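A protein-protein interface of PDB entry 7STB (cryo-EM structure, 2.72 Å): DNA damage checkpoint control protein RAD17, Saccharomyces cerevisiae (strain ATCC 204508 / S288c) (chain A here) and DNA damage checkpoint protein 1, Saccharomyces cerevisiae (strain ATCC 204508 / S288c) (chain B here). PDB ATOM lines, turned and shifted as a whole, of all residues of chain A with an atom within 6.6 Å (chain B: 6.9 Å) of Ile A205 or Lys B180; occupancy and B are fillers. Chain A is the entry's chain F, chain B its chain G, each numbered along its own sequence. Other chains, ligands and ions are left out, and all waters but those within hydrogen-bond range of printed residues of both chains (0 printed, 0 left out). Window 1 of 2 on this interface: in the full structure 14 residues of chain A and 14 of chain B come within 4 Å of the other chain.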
ATOM      1  N   SER A 165      11.189   8.987   9.370  1.00  0.00           N
ATOM      2  CA  SER A 165      11.845   8.390   8.212  1.00  0.00           C
ATOM      3  C   SER A 165      11.328   8.996   6.914  1.00  0.00           C
ATOM      4  O   SER A 165      12.109   9.297   6.004  1.00  0.00           O
ATOM      5  CB  SER A 165      11.635   6.875   8.215  1.00  0.00           C
ATOM      6  OG  SER A 165      11.968   6.316   9.473  1.00  0.00           O
ATOM      7  N   ALA A 166      10.009   9.186   6.811  1.00  0.00           N
ATOM      8  CA  ALA A 166       9.444   9.783   5.605  1.00  0.00           C
ATOM      9  C   ALA A 166       9.946  11.209   5.406  1.00  0.00           C
ATOM     10  O   ALA A 166      10.293  11.607   4.286  1.00  0.00           O
ATOM     11  CB  ALA A 166       7.918   9.757   5.675  1.00  0.00           C
ATOM     12  N   LEU A 167       9.988  11.996   6.482  1.00  0.00           N
ATOM     13  CA  LEU A 167      10.474  13.367   6.370  1.00  0.00           C
ATOM     14  C   LEU A 167      11.944  13.398   5.977  1.00  0.00           C
ATOM     15  O   LEU A 167      12.359  14.245   5.177  1.00  0.00           O
ATOM     16  CB  LEU A 167      10.249  14.116   7.684  1.00  0.00           C
ATOM     17  CG  LEU A 167       8.984  14.974   7.725  1.00  0.00           C
ATOM     18  CD1 LEU A 167       7.744  14.101   7.809  1.00  0.00           C
ATOM     19  CD2 LEU A 167       9.031  15.953   8.886  1.00  0.00           C
ATOM     20  N   ASP A 169      13.436  11.126   4.161  1.00  0.00           N
ATOM     21  CA  ASP A 169      13.468  10.766   2.748  1.00  0.00           C
ATOM     22  C   ASP A 169      13.125  11.960   1.869  1.00  0.00           C
ATOM     23  O   ASP A 169      13.778  12.197   0.847  1.00  0.00           O
ATOM     24  CB  ASP A 169      12.505   9.611   2.481  1.00  0.00           C
ATOM     25  CG  ASP A 169      12.534   9.152   1.040  1.00  0.00           C
ATOM     26  OD1 ASP A 169      13.568   9.358   0.369  1.00  0.00           O
ATOM     27  OD2 ASP A 169      11.522   8.590   0.575  1.00  0.00           O
ATOM     28  N   LEU A 170      12.097  12.724   2.248  1.00  0.00           N
ATOM     29  CA  LEU A 170      11.758  13.919   1.477  1.00  0.00           C
ATOM     30  C   LEU A 170      12.885  14.944   1.520  1.00  0.00           C
ATOM     31  O   LEU A 170      13.176  15.601   0.514  1.00  0.00           O
ATOM     32  CB  LEU A 170      10.456  14.538   1.987  1.00  0.00           C
ATOM     33  CG  LEU A 170       9.155  13.942   1.441  1.00  0.00           C
ATOM     34  CD1 LEU A 170       8.879  12.565   2.008  1.00  0.00           C
ATOM     35  CD2 LEU A 170       7.993  14.879   1.727  1.00  0.00           C
ATOM     36  N   ILE A 173      15.810  14.154  -1.014  1.00  0.00           N
ATOM     37  CA  ILE A 173      15.565  14.351  -2.439  1.00  0.00           C
ATOM     38  C   ILE A 173      15.377  15.830  -2.756  1.00  0.00           C
ATOM     39  O   ILE A 173      15.021  16.190  -3.883  1.00  0.00           O
ATOM     40  CB  ILE A 173      14.346  13.535  -2.911  1.00  0.00           C
ATOM     41  CG1 ILE A 173      13.057  14.047  -2.260  1.00  0.00           C
ATOM     42  CG2 ILE A 173      14.549  12.059  -2.601  1.00  0.00           C
ATOM     43  CD1 ILE A 173      11.809  13.347  -2.750  1.00  0.00           C
ATOM     44  N   PHE A 192      -2.890   7.442   4.040  1.00  0.00           N
ATOM     45  CA  PHE A 192      -2.208   8.688   4.371  1.00  0.00           C
ATOM     46  C   PHE A 192      -0.902   8.718   3.597  1.00  0.00           C
ATOM     47  O   PHE A 192      -0.067   7.822   3.755  1.00  0.00           O
ATOM     48  CB  PHE A 192      -1.951   8.805   5.876  1.00  0.00           C
ATOM     49  CG  PHE A 192      -1.497  10.170   6.307  1.00  0.00           C
ATOM     50  CD1 PHE A 192      -0.169  10.543   6.189  1.00  0.00           C
ATOM     51  CD2 PHE A 192      -2.398  11.083   6.824  1.00  0.00           C
ATOM     52  CE1 PHE A 192       0.252  11.798   6.583  1.00  0.00           C
ATOM     53  CE2 PHE A 192      -1.982  12.339   7.219  1.00  0.00           C
ATOM     54  CZ  PHE A 192      -0.656  12.696   7.098  1.00  0.00           C
ATOM     55  N   ALA A 193      -0.725   9.740   2.764  1.00  0.00           N
ATOM     56  CA  ALA A 193       0.415   9.801   1.863  1.00  0.00           C
ATOM     57  C   ALA A 193       1.002  11.204   1.838  1.00  0.00           C
ATOM     58  O   ALA A 193       0.303  12.201   2.041  1.00  0.00           O
ATOM     59  CB  ALA A 193       0.025   9.382   0.441  1.00  0.00           C
ATOM     60  N   LEU A 194       2.307  11.259   1.585  1.00  0.00           N
ATOM     61  CA  LEU A 194       3.031  12.499   1.341  1.00  0.00           C
ATOM     62  C   LEU A 194       3.546  12.461  -0.090  1.00  0.00           C
ATOM     63  O   LEU A 194       4.306  11.557  -0.455  1.00  0.00           O
ATOM     64  CB  LEU A 194       4.187  12.669   2.329  1.00  0.00           C
ATOM     65  CG  LEU A 194       3.809  12.960   3.783  1.00  0.00           C
ATOM     66  CD1 LEU A 194       5.047  12.935   4.666  1.00  0.00           C
ATOM     67  CD2 LEU A 194       3.096  14.295   3.904  1.00  0.00           C
ATOM     68  N   ILE A 195       3.130  13.432  -0.895  1.00  0.00           N
ATOM     69  CA  ILE A 195       3.533  13.525  -2.295  1.00  0.00           C
ATOM     70  C   ILE A 195       4.439  14.739  -2.439  1.00  0.00           C
ATOM     71  O   ILE A 195       4.022  15.871  -2.171  1.00  0.00           O
ATOM     72  CB  ILE A 195       2.323  13.614  -3.238  1.00  0.00           C
ATOM     73  CG1 ILE A 195       1.220  12.647  -2.797  1.00  0.00           C
ATOM     74  CG2 ILE A 195       2.746  13.308  -4.667  1.00  0.00           C
ATOM     75  CD1 ILE A 195      -0.067  12.793  -3.577  1.00  0.00           C
ATOM     76  N   SER A 196       5.673  14.504  -2.866  1.00  0.00           N
ATOM     77  CA  SER A 196       6.695  15.536  -2.955  1.00  0.00           C
ATOM     78  C   SER A 196       6.894  15.948  -4.405  1.00  0.00           C
ATOM     79  O   SER A 196       7.107  15.096  -5.275  1.00  0.00           O
ATOM     80  CB  SER A 196       8.018  15.043  -2.365  1.00  0.00           C
ATOM     81  OG  SER A 196       9.023  16.036  -2.474  1.00  0.00           O
ATOM     82  N   SER A 203       7.103  12.414  -6.431  1.00  0.00           N
ATOM     83  CA  SER A 203       7.320  11.169  -5.711  1.00  0.00           C
ATOM     84  C   SER A 203       6.236  11.004  -4.656  1.00  0.00           C
ATOM     85  O   SER A 203       5.646  11.983  -4.197  1.00  0.00           O
ATOM     86  CB  SER A 203       8.707  11.138  -5.058  1.00  0.00           C
ATOM     87  OG  SER A 203       8.836  12.162  -4.087  1.00  0.00           O
ATOM     88  N   LYS A 204       5.969   9.757  -4.277  1.00  0.00           N
ATOM     89  CA  LYS A 204       4.891   9.438  -3.348  1.00  0.00           C
ATOM     90  C   LYS A 204       5.407   8.506  -2.262  1.00  0.00           C
ATOM     91  O   LYS A 204       6.094   7.526  -2.561  1.00  0.00           O
ATOM     92  CB  LYS A 204       3.715   8.790  -4.086  1.00  0.00           C
ATOM     93  CG  LYS A 204       2.636   8.221  -3.180  1.00  0.00           C
ATOM     94  CD  LYS A 204       1.438   7.739  -3.983  1.00  0.00           C
ATOM     95  CE  LYS A 204       1.786   6.524  -4.829  1.00  0.00           C
ATOM     96  NZ  LYS A 204       0.577   5.870  -5.402  1.00  0.00           N
ATOM     97  N   ILE A 205       5.072   8.811  -1.010  1.00  0.00           N
ATOM     98  CA  ILE A 205       5.365   7.948   0.129  1.00  0.00           C
ATOM     99  C   ILE A 205       4.046   7.697   0.844  1.00  0.00           C
ATOM    100  O   ILE A 205       3.452   8.627   1.403  1.00  0.00           O
ATOM    101  CB  ILE A 205       6.394   8.570   1.081  1.00  0.00           C
ATOM    102  CG1 ILE A 205       7.625   9.034   0.302  1.00  0.00           C
ATOM    103  CG2 ILE A 205       6.796   7.570   2.161  1.00  0.00           C
ATOM    104  CD1 ILE A 205       8.786   9.429   1.182  1.00  0.00           C
ATOM    105  N   LYS A 206       3.590   6.449   0.843  1.00  0.00           N
ATOM    106  CA  LYS A 206       2.319   6.074   1.448  1.00  0.00           C
ATOM    107  C   LYS A 206       2.571   5.224   2.684  1.00  0.00           C
ATOM    108  O   LYS A 206       3.367   4.280   2.643  1.00  0.00           O
ATOM    109  CB  LYS A 206       1.441   5.316   0.449  1.00  0.00           C
ATOM    110  CG  LYS A 206       1.882   3.883   0.192  1.00  0.00           C
ATOM    111  CD  LYS A 206       1.236   3.300  -1.061  1.00  0.00           C
ATOM    112  CE  LYS A 206       1.686   4.009  -2.332  1.00  0.00           C
ATOM    113  NZ  LYS A 206       3.158   4.222  -2.381  1.00  0.00           N
ATOM    114  N   LEU A 207       1.891   5.569   3.791  1.00  0.00           N
ATOM    115  CA  LEU A 207       2.014   4.789   5.011  1.00  0.00           C
ATOM    116  C   LEU A 207       1.132   3.545   4.938  1.00  0.00           C
ATOM    117  O   LEU A 207       0.132   3.527   4.212  1.00  0.00           O
ATOM    118  CB  LEU A 207       1.616   5.626   6.223  1.00  0.00           C
ATOM    119  CG  LEU A 207       2.686   6.560   6.798  1.00  0.00           C
ATOM    120  CD1 LEU A 207       3.874   5.768   7.328  1.00  0.00           C
ATOM    121  CD2 LEU A 207       3.136   7.577   5.762  1.00  0.00           C
ATOM    122  N   MET A 328      -2.585   8.324  -7.460  1.00  0.00           N
ATOM    123  CA  MET A 328      -3.520   7.649  -6.569  1.00  0.00           C
ATOM    124  C   MET A 328      -4.545   6.818  -7.335  1.00  0.00           C
ATOM    125  O   MET A 328      -5.688   6.674  -6.889  1.00  0.00           O
ATOM    126  CB  MET A 328      -4.224   8.670  -5.678  1.00  0.00           C
ATOM    127  CG  MET A 328      -3.296   9.392  -4.714  1.00  0.00           C
ATOM    128  SD  MET A 328      -2.538   8.284  -3.511  1.00  0.00           S
ATOM    129  CE  MET A 328      -1.367   9.387  -2.728  1.00  0.00           C
ATOM    130  N   ILE B 138      18.154   8.189  -5.428  1.00  0.00           N
ATOM    131  CA  ILE B 138      17.026   7.282  -5.254  1.00  0.00           C
ATOM    132  C   ILE B 138      17.475   5.917  -4.736  1.00  0.00           C
ATOM    133  O   ILE B 138      16.702   5.230  -4.061  1.00  0.00           O
ATOM    134  CB  ILE B 138      16.252   7.141  -6.575  1.00  0.00           C
ATOM    135  CG1 ILE B 138      15.456   8.417  -6.860  1.00  0.00           C
ATOM    136  CG2 ILE B 138      15.322   5.934  -6.527  1.00  0.00           C
ATOM    137  CD1 ILE B 138      14.871   8.477  -8.255  1.00  0.00           C
ATOM    138  N   ARG B 140      20.120   5.245  -2.680  1.00  0.00           N
ATOM    139  CA  ARG B 140      20.875   5.234  -1.434  1.00  0.00           C
ATOM    140  C   ARG B 140      20.088   4.537  -0.328  1.00  0.00           C
ATOM    141  O   ARG B 140      18.857   4.594  -0.274  1.00  0.00           O
ATOM    142  CB  ARG B 140      21.238   6.659  -1.009  1.00  0.00           C
ATOM    143  CG  ARG B 140      20.177   7.388  -0.191  1.00  0.00           C
ATOM    144  CD  ARG B 140      18.913   7.594  -0.995  1.00  0.00           C
ATOM    145  NE  ARG B 140      17.931   8.412  -0.291  1.00  0.00           N
ATOM    146  CZ  ARG B 140      17.050   7.945   0.584  1.00  0.00           C
ATOM    147  NH1 ARG B 140      17.000   6.660   0.897  1.00  0.00           N
ATOM    148  NH2 ARG B 140      16.197   8.787   1.158  1.00  0.00           N
ATOM    149  N   PRO B 142      18.624   4.301   3.247  1.00  0.00           N
ATOM    150  CA  PRO B 142      18.287   5.303   4.265  1.00  0.00           C
ATOM    151  C   PRO B 142      19.066   5.077   5.552  1.00  0.00           C
ATOM    152  O   PRO B 142      19.390   3.945   5.921  1.00  0.00           O
ATOM    153  CB  PRO B 142      16.782   5.105   4.476  1.00  0.00           C
ATOM    154  CG  PRO B 142      16.523   3.706   4.056  1.00  0.00           C
ATOM    155  CD  PRO B 142      17.479   3.428   2.938  1.00  0.00           C
ATOM    156  N   ILE B 147      15.743  -1.513   3.524  1.00  0.00           N
ATOM    157  CA  ILE B 147      14.928  -1.712   2.332  1.00  0.00           C
ATOM    158  C   ILE B 147      14.680  -3.203   2.159  1.00  0.00           C
ATOM    159  O   ILE B 147      15.623  -4.004   2.176  1.00  0.00           O
ATOM    160  CB  ILE B 147      15.609  -1.123   1.084  1.00  0.00           C
ATOM    161  CG1 ILE B 147      15.918   0.362   1.293  1.00  0.00           C
ATOM    162  CG2 ILE B 147      14.728  -1.317  -0.144  1.00  0.00           C
ATOM    163  CD1 ILE B 147      16.806   0.958   0.220  1.00  0.00           C
ATOM    164  N   VAL B 170      10.334   3.583 -10.208  1.00  0.00           N
ATOM    165  CA  VAL B 170      11.124   3.016  -9.120  1.00  0.00           C
ATOM    166  C   VAL B 170      10.231   2.917  -7.892  1.00  0.00           C
ATOM    167  O   VAL B 170       9.684   3.928  -7.434  1.00  0.00           O
ATOM    168  CB  VAL B 170      12.372   3.862  -8.814  1.00  0.00           C
ATOM    169  CG1 VAL B 170      13.117   3.300  -7.609  1.00  0.00           C
ATOM    170  CG2 VAL B 170      13.281   3.931 -10.031  1.00  0.00           C
ATOM    171  N   VAL B 171      10.088   1.706  -7.356  1.00  0.00           N
ATOM    172  CA  VAL B 171       9.292   1.449  -6.161  1.00  0.00           C
ATOM    173  C   VAL B 171      10.222   0.881  -5.098  1.00  0.00           C
ATOM    174  O   VAL B 171      10.823  -0.182  -5.297  1.00  0.00           O
ATOM    175  CB  VAL B 171       8.129   0.484  -6.444  1.00  0.00           C
ATOM    176  CG1 VAL B 171       7.271   0.303  -5.201  1.00  0.00           C
ATOM    177  CG2 VAL B 171       7.291   0.987  -7.607  1.00  0.00           C
ATOM    178  N   ILE B 172      10.332   1.581  -3.971  1.00  0.00           N
ATOM    179  CA  ILE B 172      11.190   1.172  -2.863  1.00  0.00           C
ATOM    180  C   ILE B 172      10.302   0.855  -1.670  1.00  0.00           C
ATOM    181  O   ILE B 172       9.563   1.721  -1.192  1.00  0.00           O
ATOM    182  CB  ILE B 172      12.216   2.258  -2.504  1.00  0.00           C
ATOM    183  CG1 ILE B 172      12.878   2.814  -3.767  1.00  0.00           C
ATOM    184  CG2 ILE B 172      13.268   1.696  -1.554  1.00  0.00           C
ATOM    185  CD1 ILE B 172      13.911   3.884  -3.494  1.00  0.00           C
ATOM    186  N   GLU B 173      10.387  -0.375  -1.175  1.00  0.00           N
ATOM    187  CA  GLU B 173       9.609  -0.811  -0.024  1.00  0.00           C
ATOM    188  C   GLU B 173      10.517  -0.890   1.196  1.00  0.00           C
ATOM    189  O   GLU B 173      11.579  -1.516   1.143  1.00  0.00           O
ATOM    190  CB  GLU B 173       8.956  -2.168  -0.291  1.00  0.00           C
ATOM    191  CG  GLU B 173       7.987  -2.610   0.791  1.00  0.00           C
ATOM    192  CD  GLU B 173       7.048  -3.704   0.321  1.00  0.00           C
ATOM    193  OE1 GLU B 173       7.235  -4.205  -0.807  1.00  0.00           O
ATOM    194  OE2 GLU B 173       6.122  -4.061   1.078  1.00  0.00           O
ATOM    195  N   MET B 174      10.103  -0.248   2.281  1.00  0.00           N
ATOM    196  CA  MET B 174      10.832  -0.313   3.538  1.00  0.00           C
ATOM    197  C   MET B 174      10.391  -1.527   4.348  1.00  0.00           C
ATOM    198  O   MET B 174       9.285  -2.047   4.185  1.00  0.00           O
ATOM    199  CB  MET B 174      10.616   0.958   4.362  1.00  0.00           C
ATOM    200  CG  MET B 174      10.967   2.247   3.644  1.00  0.00           C
ATOM    201  SD  MET B 174      12.729   2.381   3.296  1.00  0.00           S
ATOM    202  CE  MET B 174      12.926   4.159   3.270  1.00  0.00           C
ATOM    203  N   ILE B 178       6.568   0.828   4.581  1.00  0.00           N
ATOM    204  CA  ILE B 178       6.454   2.099   3.875  1.00  0.00           C
ATOM    205  C   ILE B 178       6.888   1.900   2.429  1.00  0.00           C
ATOM    206  O   ILE B 178       7.820   1.140   2.143  1.00  0.00           O
ATOM    207  CB  ILE B 178       7.293   3.186   4.570  1.00  0.00           C
ATOM    208  CG1 ILE B 178       6.875   3.317   6.036  1.00  0.00           C
ATOM    209  CG2 ILE B 178       7.138   4.524   3.850  1.00  0.00           C
ATOM    210  CD1 ILE B 178       7.626   4.391   6.798  1.00  0.00           C
ATOM    211  N   VAL B 179       6.209   2.584   1.510  1.00  0.00           N
ATOM    212  CA  VAL B 179       6.460   2.457   0.080  1.00  0.00           C
ATOM    213  C   VAL B 179       6.737   3.841  -0.491  1.00  0.00           C
ATOM    214  O   VAL B 179       6.026   4.800  -0.175  1.00  0.00           O
ATOM    215  CB  VAL B 179       5.275   1.798  -0.651  1.00  0.00           C
ATOM    216  CG1 VAL B 179       5.571   1.666  -2.136  1.00  0.00           C
ATOM    217  CG2 VAL B 179       4.965   0.441  -0.042  1.00  0.00           C
ATOM    218  N   LYS B 180       7.771   3.940  -1.323  1.00  0.00           N
ATOM    219  CA  LYS B 180       8.155   5.171  -1.997  1.00  0.00           C
ATOM    220  C   LYS B 180       8.129   4.953  -3.503  1.00  0.00           C
ATOM    221  O   LYS B 180       8.561   3.904  -3.994  1.00  0.00           O
ATOM    222  CB  LYS B 180       9.553   5.627  -1.574  1.00  0.00           C
ATOM    223  CG  LYS B 180       9.671   6.035  -0.118  1.00  0.00           C
ATOM    224  CD  LYS B 180      10.905   5.439   0.545  1.00  0.00           C
ATOM    225  CE  LYS B 180      12.173   5.713  -0.255  1.00  0.00           C
ATOM    226  NZ  LYS B 180      13.407   5.527   0.553  1.00  0.00           N
ATOM    227  N   GLU B 181       7.633   5.952  -4.229  1.00  0.00           N
ATOM    228  CA  GLU B 181       7.512   5.901  -5.679  1.00  0.00           C
ATOM    229  C   GLU B 181       8.281   7.057  -6.303  1.00  0.00           C
ATOM    230  O   GLU B 181       8.197   8.196  -5.834  1.00  0.00           O
ATOM    231  CB  GLU B 181       6.043   5.963  -6.111  1.00  0.00           C
ATOM    232  CG  GLU B 181       5.168   4.861  -5.520  1.00  0.00           C
ATOM    233  CD  GLU B 181       4.849   3.752  -6.509  1.00  0.00           C
ATOM    234  OE1 GLU B 181       5.363   3.788  -7.648  1.00  0.00           O
ATOM    235  OE2 GLU B 181       4.077   2.840  -6.144  1.00  0.00           O
ATOM    236  N   TYR B 182       9.034   6.756  -7.362  1.00  0.00           N
ATOM    237  CA  TYR B 182       9.770   7.758  -8.122  1.00  0.00           C
ATOM    238  C   TYR B 182       9.570   7.514  -9.610  1.00  0.00           C
ATOM    239  O   TYR B 182       9.505   6.363 -10.057  1.00  0.00           O
ATOM    240  CB  TYR B 182      11.269   7.724  -7.801  1.00  0.00           C
ATOM    241  CG  TYR B 182      11.606   7.887  -6.338  1.00  0.00           C
ATOM    242  CD1 TYR B 182      11.769   9.146  -5.778  1.00  0.00           C
ATOM    243  CD2 TYR B 182      11.776   6.780  -5.518  1.00  0.00           C
ATOM    244  CE1 TYR B 182      12.084   9.298  -4.443  1.00  0.00           C
ATOM    245  CE2 TYR B 182      12.090   6.922  -4.183  1.00  0.00           C
ATOM    246  CZ  TYR B 182      12.243   8.183  -3.650  1.00  0.00           C
ATOM    247  OH  TYR B 182      12.557   8.329  -2.320  1.00  0.00           O
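O of Ile A205 lies within hydrogen-bond range of N of Leu A194, 2.9 Å away.
O of Ile B172 lies within hydrogen-bond range of N of Lys B180 (2.9 Å).
The backbone carbonyl oxygen (O) of Val B170 sits at hydrogen-bond distance from the backbone NH (N) of Tyr B182.
N of Ser A196 lies within hydrogen-bond range of O of Ser A203.
The side-chain carboxylate of Asp A169 is in salt-bridge range of the side-chain amino group of Lys B180, at 3.6 Å.
The side-chain carboxylate of Asp A169 lies within salt-bridge range of the guanidinium group of Arg B140 (2.8 Å).
The backbone carbonyl oxygen (O) of Val B179 lies within hydrogen-bond range of the backbone NH (N) of Lys A206, 3.1 Å away.
O of Lys A204 lies within hydrogen-bond range of N of Glu B181, 2.8 Å away.
The side-chain carboxylate of Asp A169 lies within hydrogen-bond range of the side-chain hydroxyl of Tyr B182, 3.1 Å away.
O of Glu B181 touches CB of Ser A203, 3.1 Å away.
Tyr B182 touches Ser A203.
O of Val B179 touches O of Lys A204, at 3.6 Å.
Lys A204 touches Lys B180 (O to CA, 3.2 Å).
CG2 of Ile A205 touches CG2 of Ile B178, at 3.5 Å.
CA of Ile A205 touches O of Val B179, at 3.2 Å.
Ile A205 touches Lys B180.
CG2 of Ile B178 touches O of Lys A206, 3.97 Å away.
Lys A206 touches Glu B181.
Of the printed residues of chain B, Asp A169 touches Arg B140, Lys B180 and Tyr B182.
Of the printed residues of chain B, Ser A203 touches Glu B181 and Tyr B182.
Of chain B, only Ile B178, Val B179 and Lys B180 come within 4 Å of Ile A205.
Printed residues of chain B within 4 Å of Lys A206: Ile B178, Val B179 and Glu B181.
Printed residues of chain A within 4 Å of Lys B180: Asp A169, Lys A204 and Ile A205.
Of the printed residues of chain A, Glu B181 touches Ser A203 (3.1 Å), Lys A204 (2.8 Å) and Lys A206 (3.8 Å).
Of the printed residues of chain A, Tyr B182 touches Asp A169 and Ser A203.
The nearest residue of chain B that does not touch Ile A205 is Glu B181 (5.0 Å).
The nearest residue of chain A that does not touch Lys B180 is Lys A206 (4.7 Å).
The nearest printed residue of chain A that does not touch Arg B140 is Ile A173 (5.2 Å).
Printed residues of chain B that touch a printed residue of chain A: Arg B140, Ile B178, Val B179, Lys B180, Glu B181 and Tyr B182.
Hydrophobic or aromatic side chains of chain B that line the printed part of chain A: Ile B178, Val B179 and Tyr B182.
Of the 17 printed residues of chain A, 5 touch a printed residue of chain B.
Hydrophobic or aromatic side chains of chain A that line the printed part of chain B: Ile A205.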
